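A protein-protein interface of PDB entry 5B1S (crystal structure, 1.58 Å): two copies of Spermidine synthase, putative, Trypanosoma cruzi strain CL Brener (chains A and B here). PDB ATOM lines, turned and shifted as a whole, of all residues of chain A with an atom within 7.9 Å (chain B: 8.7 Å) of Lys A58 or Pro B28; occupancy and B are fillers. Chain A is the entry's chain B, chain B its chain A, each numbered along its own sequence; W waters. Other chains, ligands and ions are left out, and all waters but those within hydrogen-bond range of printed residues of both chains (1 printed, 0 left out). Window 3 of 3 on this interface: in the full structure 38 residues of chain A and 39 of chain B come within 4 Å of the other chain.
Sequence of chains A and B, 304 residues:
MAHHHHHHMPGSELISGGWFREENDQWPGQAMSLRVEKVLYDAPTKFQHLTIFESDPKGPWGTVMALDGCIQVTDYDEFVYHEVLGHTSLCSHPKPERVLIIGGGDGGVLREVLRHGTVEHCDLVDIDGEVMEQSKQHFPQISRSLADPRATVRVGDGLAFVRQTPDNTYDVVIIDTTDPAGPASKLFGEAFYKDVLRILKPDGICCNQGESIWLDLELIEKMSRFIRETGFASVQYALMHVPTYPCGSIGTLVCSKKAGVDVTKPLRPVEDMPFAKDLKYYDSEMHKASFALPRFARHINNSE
Of chain B, only Pro B28 comes within 4 Å of Lys A58.
Of chain A, only Lys A58 (3.6 Å) and Gly A59 (3.5 Å) come within 4 Å of Pro B28.
Printed residues of chain A within 4 Å of Glu B23: Trp A19.
Of the printed residues of chain B, Leu A34 touches Gly B29 (3.5 Å) and Gln B30 (3.8 Å).
Of the printed residues of chain A, Cys B247 touches Trp A61.
Asp B25 touches none of the printed residues of chain A.
The nearest residue of chain B that does not touch Lys A58 is Gly B29 (5.6 Å).
The nearest residue of chain A that does not touch Pro B28 is Pro A60 (4.3 Å).
The nearest printed residue of chain A that does not touch Glu B23 is Ser A33 (6.9 Å).
Of the 14 printed residues of chain B, 6 touch a printed residue of chain A.
Printed residues of chain B that touch a printed residue of chain A: Glu B23, Pro B28, Gly B29, Gln B30, Ala B31 and Cys B247.
Hydrophobic or aromatic side chains of chain B that line the printed part of chain A: Pro B28 and Ala B31.
Among the printed residues, 14 pairs touch across the chains.
Among the printed residues, no Asp or Glu carboxylate lies within 4 Å of a Lys or Arg side-chain nitrogen of the other chain.
Water W1 lies within hydrogen-bond range of O of Gly B29 (2.7 Å), N of Asp A56 (2.9 Å) and O of Arg A35 (3.3 Å).
CD of Glu B23 touches CZ2 of Trp A19 (3.7 Å).
Trp A19 touches Gly B29.
Trp A19 touches Gln B30.
Ala B31 touches Trp A19.
Ser A33 touches Gln B30 (O to CA, 3.3 Å).
Leu A34 touches Gly B29 (CA to O, 3.5 Å).
Gln B30 touches Leu A34.
Gly B29 touches Asp A56 (CA to OD2, 3.9 Å).
Pro B28 touches Lys A58 (CG to O, 3.6 Å).
Cys B247 touches Trp A61 (SG to CZ2, 3.8 Å).
No position is printed for both chains.
Of the 14 pairs that touch across the chains among the printed residues, none has its exchanged pair printed and touching as well.
The backbone NH of Arg A35 is in hydrogen-bond range of the backbone carbonyl oxygen of Gly B29.
NE2 of Gln B30 lies close to NE1 of Trp A61, at 2.9 Å.
O of Ala B31 sits at hydrogen-bond distance from N of Ser A33 (2.8 Å).
OE1 of Gln B30 lies within hydrogen-bond range of SG of Cys B247 (3.5 Å).
O of Arg A35 sits at hydrogen-bond distance from N of Asp A56, 3.3 Å away.
The side-chain carboxylate of Asp A56 sits at hydrogen-bond distance from the backbone NH of Lys A58, at 2.8 Å.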
ATOM      1  N   TRP A  19      19.916  12.814 -26.219  1.00  0.00           N
ATOM      2  CA  TRP A  19      21.014  13.703 -25.847  1.00  0.00           C
ATOM      3  C   TRP A  19      22.242  12.924 -25.363  1.00  0.00           C
ATOM      4  O   TRP A  19      22.162  11.913 -24.693  1.00  0.00           O
ATOM      5  CB  TRP A  19      20.613  14.721 -24.795  1.00  0.00           C
ATOM      6  CG  TRP A  19      19.572  15.771 -25.240  1.00  0.00           C
ATOM      7  CD1 TRP A  19      18.178  15.623 -25.253  1.00  0.00           C
ATOM      8  CD2 TRP A  19      19.823  17.164 -25.517  1.00  0.00           C
ATOM      9  NE1 TRP A  19      17.587  16.839 -25.615  1.00  0.00           N
ATOM     10  CE2 TRP A  19      18.575  17.777 -25.794  1.00  0.00           C
ATOM     11  CE3 TRP A  19      21.005  17.946 -25.605  1.00  0.00           C
ATOM     12  CZ2 TRP A  19      18.456  19.151 -26.083  1.00  0.00           C
ATOM     13  CZ3 TRP A  19      20.892  19.264 -25.910  1.00  0.00           C
ATOM     14  CH2 TRP A  19      19.633  19.860 -26.213  1.00  0.00           C
ATOM     15  N   SER A  33      25.619  19.248 -22.760  1.00  0.00           N
ATOM     16  CA  SER A  33      24.757  18.309 -23.424  1.00  0.00           C
ATOM     17  C   SER A  33      24.670  18.655 -24.892  1.00  0.00           C
ATOM     18  O   SER A  33      24.512  19.848 -25.250  1.00  0.00           O
ATOM     19  CB  SER A  33      23.328  18.329 -22.823  1.00  0.00           C
ATOM     20  OG  SER A  33      23.373  18.313 -21.369  1.00  0.00           O
ATOM     21  N   LEU A  34      24.755  17.663 -25.803  1.00  0.00           N
ATOM     22  CA  LEU A  34      24.614  17.895 -27.218  1.00  0.00           C
ATOM     23  C   LEU A  34      23.533  16.924 -27.736  1.00  0.00           C
ATOM     24  O   LEU A  34      23.550  15.722 -27.337  1.00  0.00           O
ATOM     25  CB  LEU A  34      25.920  17.637 -27.969  1.00  0.00           C
ATOM     26  CG  LEU A  34      26.996  18.621 -27.582  1.00  0.00           C
ATOM     27  CD1 LEU A  34      28.333  18.138 -28.199  1.00  0.00           C
ATOM     28  CD2 LEU A  34      26.689  20.038 -28.097  1.00  0.00           C
ATOM     29  N   ARG A  35      22.635  17.382 -28.586  1.00  0.00           N
ATOM     30  CA  ARG A  35      21.609  16.516 -29.164  1.00  0.00           C
ATOM     31  C   ARG A  35      22.273  15.491 -30.086  1.00  0.00           C
ATOM     32  O   ARG A  35      23.213  15.842 -30.871  1.00  0.00           O
ATOM     33  CB  ARG A  35      20.619  17.390 -29.982  1.00  0.00           C
ATOM     34  CG  ARG A  35      19.536  16.691 -30.770  1.00  0.00           C
ATOM     35  CD  ARG A  35      18.213  16.567 -30.047  1.00  0.00           C
ATOM     36  NE  ARG A  35      17.807  15.166 -29.823  1.00  0.00           N
ATOM     37  CZ  ARG A  35      17.567  14.247 -30.770  1.00  0.00           C
ATOM     38  NH1 ARG A  35      17.710  14.500 -32.069  1.00  0.00           N
ATOM     39  NH2 ARG A  35      17.203  13.028 -30.405  1.00  0.00           N
ATOM     40  N   GLU A  37      21.737  13.118 -33.309  1.00  0.00           N
ATOM     41  CA  GLU A  37      20.971  12.838 -34.508  1.00  0.00           C
ATOM     42  C   GLU A  37      21.169  11.305 -34.816  1.00  0.00           C
ATOM     43  O   GLU A  37      20.185  10.583 -35.096  1.00  0.00           O
ATOM     44  CB  GLU A  37      21.440  13.696 -35.668  1.00  0.00           C
ATOM     45  CG  GLU A  37      20.822  13.462 -37.045  1.00  0.00           C
ATOM     46  CD  GLU A  37      19.326  13.740 -37.066  1.00  0.00           C
ATOM     47  OE1 GLU A  37      18.788  14.427 -36.167  1.00  0.00           O
ATOM     48  OE2 GLU A  37      18.714  13.152 -37.976  1.00  0.00           O
ATOM     49  N   GLU A  54      26.726  11.814 -34.716  1.00  0.00           N
ATOM     50  CA  GLU A  54      26.448  13.067 -35.459  1.00  0.00           C
ATOM     51  C   GLU A  54      25.474  13.841 -34.602  1.00  0.00           C
ATOM     52  O   GLU A  54      24.452  13.309 -34.045  1.00  0.00           O
ATOM     53  CB  GLU A  54      25.974  12.911 -36.943  1.00  0.00           C
ATOM     54  CG  GLU A  54      25.360  14.162 -37.684  1.00  0.00           C
ATOM     55  CD  GLU A  54      26.125  15.553 -37.895  1.00  0.00           C
ATOM     56  OE1 GLU A  54      27.298  15.542 -38.372  1.00  0.00           O
ATOM     57  OE2 GLU A  54      25.505  16.720 -37.712  1.00  0.00           O
ATOM     58  N   SER A  55      25.813  15.088 -34.360  1.00  0.00           N
ATOM     59  CA  SER A  55      24.918  15.934 -33.552  1.00  0.00           C
ATOM     60  C   SER A  55      23.812  16.499 -34.408  1.00  0.00           C
ATOM     61  O   SER A  55      23.794  16.376 -35.624  1.00  0.00           O
ATOM     62  CB  SER A  55      25.705  17.011 -32.792  1.00  0.00           C
ATOM     63  OG  SER A  55      26.305  17.982 -33.655  1.00  0.00           O
ATOM     64  N   ASP A  56      22.920  17.297 -33.807  1.00  0.00           N
ATOM     65  CA  ASP A  56      21.733  17.783 -34.520  1.00  0.00           C
ATOM     66  C   ASP A  56      22.115  18.701 -35.630  1.00  0.00           C
ATOM     67  O   ASP A  56      22.858  19.679 -35.424  1.00  0.00           O
ATOM     68  CB  ASP A  56      20.948  18.602 -33.468  1.00  0.00           C
ATOM     69  CG  ASP A  56      19.669  19.283 -34.015  1.00  0.00           C
ATOM     70  OD1 ASP A  56      19.350  19.124 -35.187  1.00  0.00           O
ATOM     71  OD2 ASP A  56      18.991  19.938 -33.178  1.00  0.00           O
ATOM     72  N   PRO A  57      21.634  18.410 -36.813  1.00  0.00           N
ATOM     73  CA  PRO A  57      21.934  19.213 -38.018  1.00  0.00           C
ATOM     74  C   PRO A  57      21.414  20.633 -37.923  1.00  0.00           C
ATOM     75  O   PRO A  57      21.852  21.488 -38.681  1.00  0.00           O
ATOM     76  CB  PRO A  57      21.204  18.465 -39.158  1.00  0.00           C
ATOM     77  CG  PRO A  57      20.356  17.471 -38.488  1.00  0.00           C
ATOM     78  CD  PRO A  57      20.801  17.230 -37.076  1.00  0.00           C
ATOM     79  N   LYS A  58      20.518  20.877 -36.981  1.00  0.00           N
ATOM     80  CA  LYS A  58      20.083  22.252 -36.797  1.00  0.00           C
ATOM     81  C   LYS A  58      21.058  23.068 -35.932  1.00  0.00           C
ATOM     82  O   LYS A  58      20.930  24.324 -35.827  1.00  0.00           O
ATOM     83  CB  LYS A  58      18.681  22.254 -36.142  1.00  0.00           C
ATOM     84  CG  LYS A  58      17.569  22.123 -37.172  1.00  0.00           C
ATOM     85  CD  LYS A  58      17.568  23.264 -38.200  1.00  0.00           C
ATOM     86  CE  LYS A  58      16.816  22.930 -39.489  1.00  0.00           C
ATOM     87  NZ  LYS A  58      17.592  22.074 -40.438  1.00  0.00           N
ATOM     88  N   GLY A  59      21.986  22.381 -35.293  1.00  0.00           N
ATOM     89  CA  GLY A  59      23.093  23.013 -34.526  1.00  0.00           C
ATOM     90  C   GLY A  59      24.353  22.956 -35.383  1.00  0.00           C
ATOM     91  O   GLY A  59      24.416  22.330 -36.419  1.00  0.00           O
ATOM     92  N   PRO A  60      25.436  23.613 -34.933  1.00  0.00           N
ATOM     93  CA  PRO A  60      26.589  23.752 -35.787  1.00  0.00           C
ATOM     94  C   PRO A  60      27.696  22.714 -35.558  1.00  0.00           C
ATOM     95  O   PRO A  60      28.717  22.774 -36.229  1.00  0.00           O
ATOM     96  CB  PRO A  60      27.137  25.124 -35.284  1.00  0.00           C
ATOM     97  CG  PRO A  60      26.862  25.098 -33.798  1.00  0.00           C
ATOM     98  CD  PRO A  60      25.423  24.594 -33.821  1.00  0.00           C
ATOM     99  N   TRP A  61      27.515  21.817 -34.589  1.00  0.00           N
ATOM    100  CA  TRP A  61      28.647  21.074 -34.007  1.00  0.00           C
ATOM    101  C   TRP A  61      29.137  19.932 -34.850  1.00  0.00           C
ATOM    102  O   TRP A  61      30.316  19.599 -34.755  1.00  0.00           O
ATOM    103  CB  TRP A  61      28.326  20.543 -32.583  1.00  0.00           C
ATOM    104  CG  TRP A  61      27.980  21.684 -31.717  1.00  0.00           C
ATOM    105  CD1 TRP A  61      26.724  22.124 -31.387  1.00  0.00           C
ATOM    106  CD2 TRP A  61      28.893  22.690 -31.245  1.00  0.00           C
ATOM    107  NE1 TRP A  61      26.802  23.333 -30.700  1.00  0.00           N
ATOM    108  CE2 TRP A  61      28.127  23.688 -30.598  1.00  0.00           C
ATOM    109  CE3 TRP A  61      30.293  22.799 -31.239  1.00  0.00           C
ATOM    110  CZ2 TRP A  61      28.687  24.795 -30.016  1.00  0.00           C
ATOM    111  CZ3 TRP A  61      30.856  23.939 -30.661  1.00  0.00           C
ATOM    112  CH2 TRP A  61      30.065  24.907 -30.082  1.00  0.00           C
ATOM    113  N   GLU B  22      19.546  23.975 -20.099  1.00  0.00           N
ATOM    114  CA  GLU B  22      19.423  25.273 -20.725  1.00  0.00           C
ATOM    115  C   GLU B  22      19.165  25.062 -22.191  1.00  0.00           C
ATOM    116  O   GLU B  22      19.933  25.437 -23.092  1.00  0.00           O
ATOM    117  CB  GLU B  22      20.698  26.065 -20.469  1.00  0.00           C
ATOM    118  CG  GLU B  22      20.408  27.568 -20.650  1.00  0.00           C
ATOM    119  CD  GLU B  22      21.656  28.414 -20.757  1.00  0.00           C
ATOM    120  OE1 GLU B  22      22.701  27.898 -21.216  1.00  0.00           O
ATOM    121  OE2 GLU B  22      21.565  29.632 -20.400  1.00  0.00           O
ATOM    122  N   GLU B  23      18.064  24.399 -22.499  1.00  0.00           N
ATOM    123  CA  GLU B  23      17.645  24.161 -23.890  1.00  0.00           C
ATOM    124  C   GLU B  23      16.969  25.423 -24.410  1.00  0.00           C
ATOM    125  O   GLU B  23      16.111  25.964 -23.693  1.00  0.00           O
ATOM    126  CB  GLU B  23      16.633  22.993 -23.903  1.00  0.00           C
ATOM    127  CG  GLU B  23      17.223  21.759 -23.290  1.00  0.00           C
ATOM    128  CD  GLU B  23      16.300  20.545 -23.419  1.00  0.00           C
ATOM    129  OE1 GLU B  23      15.328  20.684 -24.187  1.00  0.00           O
ATOM    130  OE2 GLU B  23      16.574  19.496 -22.815  1.00  0.00           O
ATOM    131  N   ASN B  24      17.298  25.872 -25.629  1.00  0.00           N
ATOM    132  CA  ASN B  24      16.771  27.124 -26.158  1.00  0.00           C
ATOM    133  C   ASN B  24      16.943  27.166 -27.646  1.00  0.00           C
ATOM    134  O   ASN B  24      18.001  26.765 -28.129  1.00  0.00           O
ATOM    135  CB  ASN B  24      17.530  28.292 -25.524  1.00  0.00           C
ATOM    136  CG  ASN B  24      16.686  29.578 -25.563  1.00  0.00           C
ATOM    137  OD1 ASN B  24      16.584  30.217 -26.612  1.00  0.00           O
ATOM    138  ND2 ASN B  24      16.166  29.958 -24.436  1.00  0.00           N
ATOM    139  N   ASP B  25      15.941  27.608 -28.408  1.00  0.00           N
ATOM    140  CA  ASP B  25      16.119  27.719 -29.780  1.00  0.00           C
ATOM    141  C   ASP B  25      17.104  28.811 -30.225  1.00  0.00           C
ATOM    142  O   ASP B  25      17.429  28.935 -31.401  1.00  0.00           O
ATOM    143  CB  ASP B  25      14.775  27.768 -30.559  1.00  0.00           C
ATOM    144  CG  ASP B  25      13.902  28.866 -30.119  1.00  0.00           C
ATOM    145  OD1 ASP B  25      14.424  29.978 -29.837  1.00  0.00           O
ATOM    146  OD2 ASP B  25      12.652  28.646 -30.112  1.00  0.00           O
ATOM    147  N   GLN B  26      17.592  29.600 -29.248  1.00  0.00           N
ATOM    148  CA  GLN B  26      18.673  30.551 -29.557  1.00  0.00           C
ATOM    149  C   GLN B  26      20.025  29.865 -29.670  1.00  0.00           C
ATOM    150  O   GLN B  26      21.002  30.476 -30.187  1.00  0.00           O
ATOM    151  CB  GLN B  26      18.719  31.684 -28.527  1.00  0.00           C
ATOM    152  CG  GLN B  26      17.484  32.591 -28.659  1.00  0.00           C
ATOM    153  CD  GLN B  26      17.397  33.623 -27.580  1.00  0.00           C
ATOM    154  OE1 GLN B  26      17.492  34.843 -27.900  1.00  0.00           O
ATOM    155  NE2 GLN B  26      17.108  33.194 -26.351  1.00  0.00           N
ATOM    156  N   TRP B  27      20.089  28.617 -29.215  1.00  0.00           N
ATOM    157  CA  TRP B  27      21.297  27.787 -29.413  1.00  0.00           C
ATOM    158  C   TRP B  27      20.891  26.333 -29.658  1.00  0.00           C
ATOM    159  O   TRP B  27      21.034  25.463 -28.776  1.00  0.00           O
ATOM    160  CB  TRP B  27      22.241  27.892 -28.236  1.00  0.00           C
ATOM    161  CG  TRP B  27      21.633  28.023 -26.871  1.00  0.00           C
ATOM    162  CD1 TRP B  27      21.249  27.062 -26.039  1.00  0.00           C
ATOM    163  CD2 TRP B  27      21.343  29.268 -26.212  1.00  0.00           C
ATOM    164  NE1 TRP B  27      20.781  27.602 -24.828  1.00  0.00           N
ATOM    165  CE2 TRP B  27      20.797  28.970 -24.955  1.00  0.00           C
ATOM    166  CE3 TRP B  27      21.540  30.578 -26.566  1.00  0.00           C
ATOM    167  CZ2 TRP B  27      20.395  29.969 -24.048  1.00  0.00           C
ATOM    168  CZ3 TRP B  27      21.115  31.602 -25.657  1.00  0.00           C
ATOM    169  CH2 TRP B  27      20.547  31.269 -24.431  1.00  0.00           C
ATOM    170  N   PRO B  28      20.370  26.100 -30.867  1.00  0.00           N
ATOM    171  CA  PRO B  28      19.831  24.767 -31.081  1.00  0.00           C
ATOM    172  C   PRO B  28      20.854  23.660 -30.958  1.00  0.00           C
ATOM    173  O   PRO B  28      22.029  23.847 -31.333  1.00  0.00           O
ATOM    174  CB  PRO B  28      19.315  24.808 -32.538  1.00  0.00           C
ATOM    175  CG  PRO B  28      19.561  26.193 -33.099  1.00  0.00           C
ATOM    176  CD  PRO B  28      20.369  26.953 -32.078  1.00  0.00           C
ATOM    177  N   GLY B  29      20.350  22.551 -30.439  1.00  0.00           N
ATOM    178  CA  GLY B  29      21.223  21.354 -30.318  1.00  0.00           C
ATOM    179  C   GLY B  29      22.196  21.250 -29.168  1.00  0.00           C
ATOM    180  O   GLY B  29      22.975  20.287 -29.127  1.00  0.00           O
ATOM    181  N   GLN B  30      22.252  22.201 -28.239  1.00  0.00           N
ATOM    182  CA  GLN B  30      23.155  22.152 -27.184  1.00  0.00           C
ATOM    183  C   GLN B  30      22.436  22.655 -25.952  1.00  0.00           C
ATOM    184  O   GLN B  30      21.444  23.431 -26.025  1.00  0.00           O
ATOM    185  CB  GLN B  30      24.392  23.041 -27.481  1.00  0.00           C
ATOM    186  CG  GLN B  30      24.027  24.545 -27.582  1.00  0.00           C
ATOM    187  CD  GLN B  30      25.227  25.388 -28.006  1.00  0.00           C
ATOM    188  OE1 GLN B  30      25.877  26.034 -27.149  1.00  0.00           O
ATOM    189  NE2 GLN B  30      25.460  25.438 -29.253  1.00  0.00           N
ATOM    190  N   ALA B  31      22.992  22.265 -24.824  1.00  0.00           N
ATOM    191  CA  ALA B  31      22.445  22.789 -23.545  1.00  0.00           C
ATOM    192  C   ALA B  31      23.413  22.547 -22.426  1.00  0.00           C
ATOM    193  O   ALA B  31      23.878  21.366 -22.165  1.00  0.00           O
ATOM    194  CB  ALA B  31      21.084  22.104 -23.247  1.00  0.00           C
ATOM    195  N   LEU B 215      27.900  31.664 -31.814  1.00  0.00           N
ATOM    196  CA  LEU B 215      26.424  31.573 -32.084  1.00  0.00           C
ATOM    197  C   LEU B 215      25.809  32.742 -32.814  1.00  0.00           C
ATOM    198  O   LEU B 215      24.723  32.594 -33.435  1.00  0.00           O
ATOM    199  CB  LEU B 215      25.722  31.447 -30.696  1.00  0.00           C
ATOM    200  CG  LEU B 215      26.132  30.228 -29.834  1.00  0.00           C
ATOM    201  CD1 LEU B 215      25.608  30.307 -28.380  1.00  0.00           C
ATOM    202  CD2 LEU B 215      25.692  28.918 -30.493  1.00  0.00           C
ATOM    203  N   ASP B 216      26.433  33.905 -32.698  1.00  0.00           N
ATOM    204  CA  ASP B 216      25.759  35.146 -33.028  1.00  0.00           C
ATOM    205  C   ASP B 216      26.632  36.020 -33.890  1.00  0.00           C
ATOM    206  O   ASP B 216      26.486  37.251 -33.870  1.00  0.00           O
ATOM    207  CB  ASP B 216      25.388  35.910 -31.711  1.00  0.00           C
ATOM    208  CG  ASP B 216      24.561  35.112 -30.817  1.00  0.00           C
ATOM    209  OD1 ASP B 216      23.430  34.821 -31.258  1.00  0.00           O
ATOM    210  OD2 ASP B 216      24.956  34.742 -29.670  1.00  0.00           O
ATOM    211  N   PRO B 246      26.296  30.566 -22.902  1.00  0.00           N
ATOM    212  CA  PRO B 246      26.347  29.550 -23.937  1.00  0.00           C
ATOM    213  C   PRO B 246      27.635  29.560 -24.720  1.00  0.00           C
ATOM    214  O   PRO B 246      28.100  30.607 -25.093  1.00  0.00           O
ATOM    215  CB  PRO B 246      25.144  29.891 -24.792  1.00  0.00           C
ATOM    216  CG  PRO B 246      24.125  30.345 -23.722  1.00  0.00           C
ATOM    217  CD  PRO B 246      24.999  31.280 -22.900  1.00  0.00           C
ATOM    218  N   CYS B 247      28.220  28.388 -24.826  1.00  0.00           N
ATOM    219  CA  CYS B 247      29.547  28.173 -25.384  1.00  0.00           C
ATOM    220  C   CYS B 247      30.726  28.606 -24.536  1.00  0.00           C
ATOM    221  O   CYS B 247      31.865  28.475 -25.017  1.00  0.00           O
ATOM    222  CB  CYS B 247      29.659  28.714 -26.784  1.00  0.00           C
ATOM    223  SG  CYS B 247      28.603  28.038 -28.083  1.00  0.00           S
HETATM  224  O   HOH W   1      23.510  19.047 -31.521  1.00  0.00           O
